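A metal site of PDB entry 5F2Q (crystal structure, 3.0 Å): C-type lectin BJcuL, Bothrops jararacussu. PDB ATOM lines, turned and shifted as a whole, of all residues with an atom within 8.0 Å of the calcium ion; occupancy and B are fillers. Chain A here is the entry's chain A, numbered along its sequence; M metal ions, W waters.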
ATOM      1  N   TRP A  79     -28.951   0.245  12.323  1.00  0.00           N
ATOM      2  CA  TRP A  79     -28.144  -0.932  12.002  1.00  0.00           C
ATOM      3  C   TRP A  79     -27.960  -1.774  13.265  1.00  0.00           C
ATOM      4  O   TRP A  79     -27.268  -1.355  14.205  1.00  0.00           O
ATOM      5  CB  TRP A  79     -26.801  -0.488  11.416  1.00  0.00           C
ATOM      6  CG  TRP A  79     -26.952   0.398  10.206  1.00  0.00           C
ATOM      7  CD1 TRP A  79     -27.013   1.760  10.197  1.00  0.00           C
ATOM      8  CD2 TRP A  79     -27.096  -0.021   8.848  1.00  0.00           C
ATOM      9  NE1 TRP A  79     -27.164   2.219   8.912  1.00  0.00           N
ATOM     10  CE2 TRP A  79     -27.219   1.142   8.062  1.00  0.00           C
ATOM     11  CE3 TRP A  79     -27.116  -1.271   8.211  1.00  0.00           C
ATOM     12  CZ2 TRP A  79     -27.359   1.101   6.674  1.00  0.00           C
ATOM     13  CZ3 TRP A  79     -27.263  -1.312   6.835  1.00  0.00           C
ATOM     14  CH2 TRP A  79     -27.385  -0.127   6.083  1.00  0.00           C
ATOM     15  N   TRP A  92     -17.257   2.387   7.195  1.00  0.00           N
ATOM     16  CA  TRP A  92     -17.933   2.439   5.910  1.00  0.00           C
ATOM     17  C   TRP A  92     -16.959   2.716   4.766  1.00  0.00           C
ATOM     18  O   TRP A  92     -15.855   3.217   4.971  1.00  0.00           O
ATOM     19  CB  TRP A  92     -19.025   3.513   5.924  1.00  0.00           C
ATOM     20  CG  TRP A  92     -20.199   3.203   6.788  1.00  0.00           C
ATOM     21  CD1 TRP A  92     -20.596   3.888   7.898  1.00  0.00           C
ATOM     22  CD2 TRP A  92     -21.143   2.143   6.605  1.00  0.00           C
ATOM     23  NE1 TRP A  92     -21.735   3.308   8.426  1.00  0.00           N
ATOM     24  CE2 TRP A  92     -22.082   2.237   7.655  1.00  0.00           C
ATOM     25  CE3 TRP A  92     -21.289   1.118   5.667  1.00  0.00           C
ATOM     26  CZ2 TRP A  92     -23.149   1.352   7.779  1.00  0.00           C
ATOM     27  CZ3 TRP A  92     -22.340   0.232   5.800  1.00  0.00           C
ATOM     28  CH2 TRP A  92     -23.265   0.357   6.843  1.00  0.00           C
ATOM     29  N   ASP A  93     -17.398   2.378   3.560  1.00  0.00           N
ATOM     30  CA  ASP A  93     -16.642   2.699   2.348  1.00  0.00           C
ATOM     31  C   ASP A  93     -16.976   4.139   1.931  1.00  0.00           C
ATOM     32  O   ASP A  93     -17.620   4.881   2.666  1.00  0.00           O
ATOM     33  CB  ASP A  93     -16.958   1.699   1.248  1.00  0.00           C
ATOM     34  CG  ASP A  93     -15.869   1.619   0.190  1.00  0.00           C
ATOM     35  OD1 ASP A  93     -15.006   2.531   0.158  1.00  0.00           O
ATOM     36  OD2 ASP A  93     -15.864   0.657  -0.605  1.00  0.00           O
ATOM     37  N   LYS A  94     -16.539   4.524   0.740  1.00  0.00           N
ATOM     38  CA  LYS A  94     -16.802   5.875   0.259  1.00  0.00           C
ATOM     39  C   LYS A  94     -18.299   6.101   0.122  1.00  0.00           C
ATOM     40  O   LYS A  94     -18.975   5.402  -0.625  1.00  0.00           O
ATOM     41  CB  LYS A  94     -16.097   6.104  -1.075  1.00  0.00           C
ATOM     42  CG  LYS A  94     -16.081   7.568  -1.526  1.00  0.00           C
ATOM     43  CD  LYS A  94     -15.467   7.753  -2.907  1.00  0.00           C
ATOM     44  CE  LYS A  94     -15.334   9.236  -3.270  1.00  0.00           C
ATOM     45  NZ  LYS A  94     -14.910   9.465  -4.676  1.00  0.00           N
ATOM     46  N   ASN A  95     -18.815   7.083   0.878  1.00  0.00           N
ATOM     47  CA  ASN A  95     -20.196   7.543   0.738  1.00  0.00           C
ATOM     48  C   ASN A  95     -21.200   6.432   1.032  1.00  0.00           C
ATOM     49  O   ASN A  95     -22.297   6.415   0.468  1.00  0.00           O
ATOM     50  CB  ASN A  95     -20.449   8.114  -0.660  1.00  0.00           C
ATOM     51  CG  ASN A  95     -19.590   9.322  -0.968  1.00  0.00           C
ATOM     52  OD1 ASN A  95     -19.263  10.124  -0.086  1.00  0.00           O
ATOM     53  ND2 ASN A  95     -19.230   9.472  -2.239  1.00  0.00           N
ATOM     54  N   GLN A  96     -20.840   5.501   1.914  1.00  0.00           N
ATOM     55  CA  GLN A  96     -21.789   4.492   2.392  1.00  0.00           C
ATOM     56  C   GLN A  96     -22.188   4.842   3.815  1.00  0.00           C
ATOM     57  O   GLN A  96     -21.421   5.491   4.527  1.00  0.00           O
ATOM     58  CB  GLN A  96     -21.175   3.092   2.325  1.00  0.00           C
ATOM     59  CG  GLN A  96     -20.612   2.719   0.952  1.00  0.00           C
ATOM     60  CD  GLN A  96     -21.659   2.803  -0.153  1.00  0.00           C
ATOM     61  OE1 GLN A  96     -22.729   2.199  -0.064  1.00  0.00           O
ATOM     62  NE2 GLN A  96     -21.332   3.546  -1.203  1.00  0.00           N
ATOM     63  N   PRO A  97     -23.383   4.423   4.251  1.00  0.00           N
ATOM     64  CA  PRO A  97     -24.403   3.672   3.500  1.00  0.00           C
ATOM     65  C   PRO A  97     -25.255   4.599   2.631  1.00  0.00           C
ATOM     66  O   PRO A  97     -25.347   5.783   2.951  1.00  0.00           O
ATOM     67  CB  PRO A  97     -25.234   3.041   4.615  1.00  0.00           C
ATOM     68  CG  PRO A  97     -25.202   4.080   5.707  1.00  0.00           C
ATOM     69  CD  PRO A  97     -23.852   4.762   5.606  1.00  0.00           C
ATOM     70  N   ASP A  98     -25.859   4.081   1.564  1.00  0.00           N
ATOM     71  CA  ASP A  98     -26.606   4.929   0.643  1.00  0.00           C
ATOM     72  C   ASP A  98     -27.966   4.389   0.207  1.00  0.00           C
ATOM     73  O   ASP A  98     -28.728   5.151  -0.382  1.00  0.00           O
ATOM     74  CB  ASP A  98     -25.763   5.217  -0.606  1.00  0.00           C
ATOM     75  CG  ASP A  98     -25.251   3.953  -1.282  1.00  0.00           C
ATOM     76  OD1 ASP A  98     -25.639   2.831  -0.875  1.00  0.00           O
ATOM     77  OD2 ASP A  98     -24.457   4.083  -2.246  1.00  0.00           O
ATOM     78  N   HIS A  99     -28.293   3.130   0.468  1.00  0.00           N
ATOM     79  CA  HIS A  99     -29.574   2.562   0.055  1.00  0.00           C
ATOM     80  C   HIS A  99     -29.803   2.767  -1.445  1.00  0.00           C
ATOM     81  O   HIS A  99     -30.809   3.344  -1.869  1.00  0.00           O
ATOM     82  CB  HIS A  99     -30.740   3.173   0.843  1.00  0.00           C
ATOM     83  CG  HIS A  99     -30.789   2.787   2.288  1.00  0.00           C
ATOM     84  ND1 HIS A  99     -31.638   3.398   3.179  1.00  0.00           N
ATOM     85  CD2 HIS A  99     -30.100   1.856   2.990  1.00  0.00           C
ATOM     86  CE1 HIS A  99     -31.477   2.864   4.379  1.00  0.00           C
ATOM     87  NE2 HIS A  99     -30.550   1.917   4.290  1.00  0.00           N
ATOM     88  N   TYR A 100     -28.863   2.294  -2.263  1.00  0.00           N
ATOM     89  CA  TYR A 100     -28.995   2.517  -3.696  1.00  0.00           C
ATOM     90  C   TYR A 100     -30.233   1.791  -4.207  1.00  0.00           C
ATOM     91  O   TYR A 100     -30.405   0.589  -4.000  1.00  0.00           O
ATOM     92  CB  TYR A 100     -27.757   2.038  -4.456  1.00  0.00           C
ATOM     93  CG  TYR A 100     -27.765   2.515  -5.894  1.00  0.00           C
ATOM     94  CD1 TYR A 100     -27.813   3.865  -6.194  1.00  0.00           C
ATOM     95  CD2 TYR A 100     -27.725   1.608  -6.958  1.00  0.00           C
ATOM     96  CE1 TYR A 100     -27.830   4.315  -7.497  1.00  0.00           C
ATOM     97  CE2 TYR A 100     -27.741   2.051  -8.277  1.00  0.00           C
ATOM     98  CZ  TYR A 100     -27.791   3.412  -8.537  1.00  0.00           C
ATOM     99  OH  TYR A 100     -27.804   3.870  -9.837  1.00  0.00           O
ATOM    100  N   GLN A 101     -31.107   2.541  -4.882  1.00  0.00           N
ATOM    101  CA  GLN A 101     -32.410   2.072  -5.333  1.00  0.00           C
ATOM    102  C   GLN A 101     -33.326   1.691  -4.170  1.00  0.00           C
ATOM    103  O   GLN A 101     -34.350   1.028  -4.376  1.00  0.00           O
ATOM    104  CB  GLN A 101     -32.286   0.875  -6.297  1.00  0.00           C
ATOM    105  CG  GLN A 101     -31.617   1.234  -7.627  1.00  0.00           C
ATOM    106  CD  GLN A 101     -31.703   0.110  -8.645  1.00  0.00           C
ATOM    107  OE1 GLN A 101     -31.035  -0.923  -8.504  1.00  0.00           O
ATOM    108  NE2 GLN A 101     -32.521   0.295  -9.676  1.00  0.00           N
ATOM    109  N   GLU A 104     -31.151  -1.776  -0.582  1.00  0.00           N
ATOM    110  CA  GLU A 104     -29.943  -2.264   0.082  1.00  0.00           C
ATOM    111  C   GLU A 104     -30.108  -2.096   1.590  1.00  0.00           C
ATOM    112  O   GLU A 104     -30.281  -0.979   2.076  1.00  0.00           O
ATOM    113  CB  GLU A 104     -28.706  -1.510  -0.410  1.00  0.00           C
ATOM    114  CG  GLU A 104     -28.406  -1.669  -1.893  1.00  0.00           C
ATOM    115  CD  GLU A 104     -27.143  -0.932  -2.329  1.00  0.00           C
ATOM    116  OE1 GLU A 104     -26.691  -0.039  -1.593  1.00  0.00           O
ATOM    117  OE2 GLU A 104     -26.609  -1.256  -3.412  1.00  0.00           O
ATOM    118  N   PHE A 105     -30.030  -3.216   2.324  1.00  0.00           N
ATOM    119  CA  PHE A 105     -30.213  -3.190   3.771  1.00  0.00           C
ATOM    120  C   PHE A 105     -29.282  -4.106   4.546  1.00  0.00           C
ATOM    121  O   PHE A 105     -29.246  -4.013   5.779  1.00  0.00           O
ATOM    122  CB  PHE A 105     -31.663  -3.533   4.125  1.00  0.00           C
ATOM    123  CG  PHE A 105     -32.678  -2.637   3.473  1.00  0.00           C
ATOM    124  CD1 PHE A 105     -32.746  -1.296   3.815  1.00  0.00           C
ATOM    125  CD2 PHE A 105     -33.564  -3.127   2.538  1.00  0.00           C
ATOM    126  CE1 PHE A 105     -33.676  -0.463   3.223  1.00  0.00           C
ATOM    127  CE2 PHE A 105     -34.491  -2.307   1.939  1.00  0.00           C
ATOM    128  CZ  PHE A 105     -34.551  -0.970   2.279  1.00  0.00           C
ATOM    129  N   CYS A 106     -28.547  -5.002   3.891  1.00  0.00           N
ATOM    130  CA  CYS A 106     -27.556  -5.855   4.546  1.00  0.00           C
ATOM    131  C   CYS A 106     -26.158  -5.377   4.177  1.00  0.00           C
ATOM    132  O   CYS A 106     -25.954  -4.736   3.143  1.00  0.00           O
ATOM    133  CB  CYS A 106     -27.749  -7.321   4.142  1.00  0.00           C
ATOM    134  SG  CYS A 106     -29.313  -8.047   4.717  1.00  0.00           S
ATOM    135  N   GLU A 108     -21.922  -5.840   3.661  1.00  0.00           N
ATOM    136  CA  GLU A 108     -20.874  -6.719   3.165  1.00  0.00           C
ATOM    137  C   GLU A 108     -19.518  -6.052   3.351  1.00  0.00           C
ATOM    138  O   GLU A 108     -19.426  -4.838   3.543  1.00  0.00           O
ATOM    139  CB  GLU A 108     -21.084  -7.061   1.684  1.00  0.00           C
ATOM    140  CG  GLU A 108     -20.942  -5.847   0.762  1.00  0.00           C
ATOM    141  CD  GLU A 108     -21.276  -6.152  -0.687  1.00  0.00           C
ATOM    142  OE1 GLU A 108     -21.671  -7.301  -0.973  1.00  0.00           O
ATOM    143  OE2 GLU A 108     -21.148  -5.240  -1.527  1.00  0.00           O
ATOM    144  N   TRP A 118     -17.020  -1.102   4.653  1.00  0.00           N
ATOM    145  CA  TRP A 118     -18.333  -1.712   4.560  1.00  0.00           C
ATOM    146  C   TRP A 118     -19.156  -1.035   3.469  1.00  0.00           C
ATOM    147  O   TRP A 118     -18.969   0.139   3.155  1.00  0.00           O
ATOM    148  CB  TRP A 118     -19.080  -1.617   5.886  1.00  0.00           C
ATOM    149  CG  TRP A 118     -18.325  -2.122   7.085  1.00  0.00           C
ATOM    150  CD1 TRP A 118     -17.150  -2.818   7.090  1.00  0.00           C
ATOM    151  CD2 TRP A 118     -18.709  -1.972   8.459  1.00  0.00           C
ATOM    152  NE1 TRP A 118     -16.770  -3.106   8.384  1.00  0.00           N
ATOM    153  CE2 TRP A 118     -17.712  -2.597   9.243  1.00  0.00           C
ATOM    154  CE3 TRP A 118     -19.785  -1.365   9.111  1.00  0.00           C
ATOM    155  CZ2 TRP A 118     -17.771  -2.636  10.632  1.00  0.00           C
ATOM    156  CZ3 TRP A 118     -19.838  -1.403  10.489  1.00  0.00           C
ATOM    157  CH2 TRP A 118     -18.832  -2.032  11.236  1.00  0.00           C
ATOM    158  N   ASN A 119     -20.093  -1.809   2.901  1.00  0.00           N
ATOM    159  CA  ASN A 119     -21.055  -1.300   1.940  1.00  0.00           C
ATOM    160  C   ASN A 119     -22.405  -1.957   2.189  1.00  0.00           C
ATOM    161  O   ASN A 119     -22.474  -3.168   2.426  1.00  0.00           O
ATOM    162  CB  ASN A 119     -20.641  -1.585   0.493  1.00  0.00           C
ATOM    163  CG  ASN A 119     -21.718  -1.209  -0.514  1.00  0.00           C
ATOM    164  OD1 ASN A 119     -22.231  -0.097  -0.495  1.00  0.00           O
ATOM    165  ND2 ASN A 119     -22.069  -2.157  -1.379  1.00  0.00           N
ATOM    166  N   ASP A 120     -23.471  -1.160   2.135  1.00  0.00           N
ATOM    167  CA  ASP A 120     -24.821  -1.709   2.202  1.00  0.00           C
ATOM    168  C   ASP A 120     -25.215  -2.239   0.823  1.00  0.00           C
ATOM    169  O   ASP A 120     -25.019  -1.557  -0.200  1.00  0.00           O
ATOM    170  CB  ASP A 120     -25.818  -0.666   2.689  1.00  0.00           C
ATOM    171  CG  ASP A 120     -25.894   0.552   1.791  1.00  0.00           C
ATOM    172  OD1 ASP A 120     -24.845   0.982   1.273  1.00  0.00           O
ATOM    173  OD2 ASP A 120     -27.014   1.076   1.612  1.00  0.00           O
ATOM    174  N   GLN A 121     -25.767  -3.443   0.797  1.00  0.00           N
ATOM    175  CA  GLN A 121     -26.019  -4.200  -0.421  1.00  0.00           C
ATOM    176  C   GLN A 121     -27.387  -4.865  -0.299  1.00  0.00           C
ATOM    177  O   GLN A 121     -27.904  -5.048   0.802  1.00  0.00           O
ATOM    178  CB  GLN A 121     -24.914  -5.257  -0.642  1.00  0.00           C
ATOM    179  CG  GLN A 121     -24.999  -6.077  -1.932  1.00  0.00           C
ATOM    180  CD  GLN A 121     -24.381  -5.365  -3.118  1.00  0.00           C
ATOM    181  OE1 GLN A 121     -24.956  -4.433  -3.684  1.00  0.00           O
ATOM    182  NE2 GLN A 121     -23.184  -5.809  -3.506  1.00  0.00           N
ATOM    183  N   VAL A 122     -27.960  -5.225  -1.446  1.00  0.00           N
ATOM    184  CA  VAL A 122     -29.259  -5.902  -1.440  1.00  0.00           C
ATOM    185  C   VAL A 122     -29.126  -7.204  -0.682  1.00  0.00           C
ATOM    186  O   VAL A 122     -28.252  -8.031  -0.952  1.00  0.00           O
ATOM    187  CB  VAL A 122     -29.748  -6.127  -2.876  1.00  0.00           C
ATOM    188  CG1 VAL A 122     -31.011  -7.002  -2.897  1.00  0.00           C
ATOM    189  CG2 VAL A 122     -30.027  -4.794  -3.558  1.00  0.00           C
HETATM  190 CA    CA M   1     -24.437   0.670  -0.957  1.00  0.00          CA
HETATM  191  O   HOH W   1     -23.967  -0.484  -3.665  1.00  0.00           O
HETATM  192  O   HOH W   2     -23.586   1.596  -3.029  1.00  0.00           O
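OD1 of Asp 120 is bound to the calcium ion (2.3 Å). OD1 of Asn 119 binds the calcium ion. The calcium ion is bound by the backbone carbonyl oxygen (O) of Asp 120, 2.4 Å away. Water W2 binds the calcium ion (2.4 Å). The calcium ion is bound by OE1 of Glu 104, 2.4 Å away. The side-chain amide oxygen (OE1) of Gln 96 binds the calcium ion, 2.5 Å away. The calcium ion is bound by OD1 of Asp 98. The calcium ion has seven donor atoms within binding distance. Slightly farther from the calcium ion lies water W1 (3.0 Å).
Five residues have an atom within 4 Å of the calcium ion: Gln 96, Asp 98, Glu 104, Asn 119 and Asp 120.
OD2 of Asp 120 lies within hydrogen-bond range of N of His 99 (2.7 Å). O of Asn 119 sits at hydrogen-bond distance from N of Glu 108 (3.0 Å). The side-chain carboxylate (OE1) of Glu 104 lies close to the backbone NH (N) of Tyr 100. The side-chain amide nitrogen (NE2) of Gln 96 sits at hydrogen-bond distance from the backbone carbonyl oxygen (O) of Lys 94, 3.1 Å away.
Water W2 lies within hydrogen-bond range of OD2 of Asp 98 and NE2 of Gln 96. Water W1 lies within hydrogen-bond range of OE2 of Glu 104 (2.8 Å) and ND2 of Asn 119 (3.4 Å).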
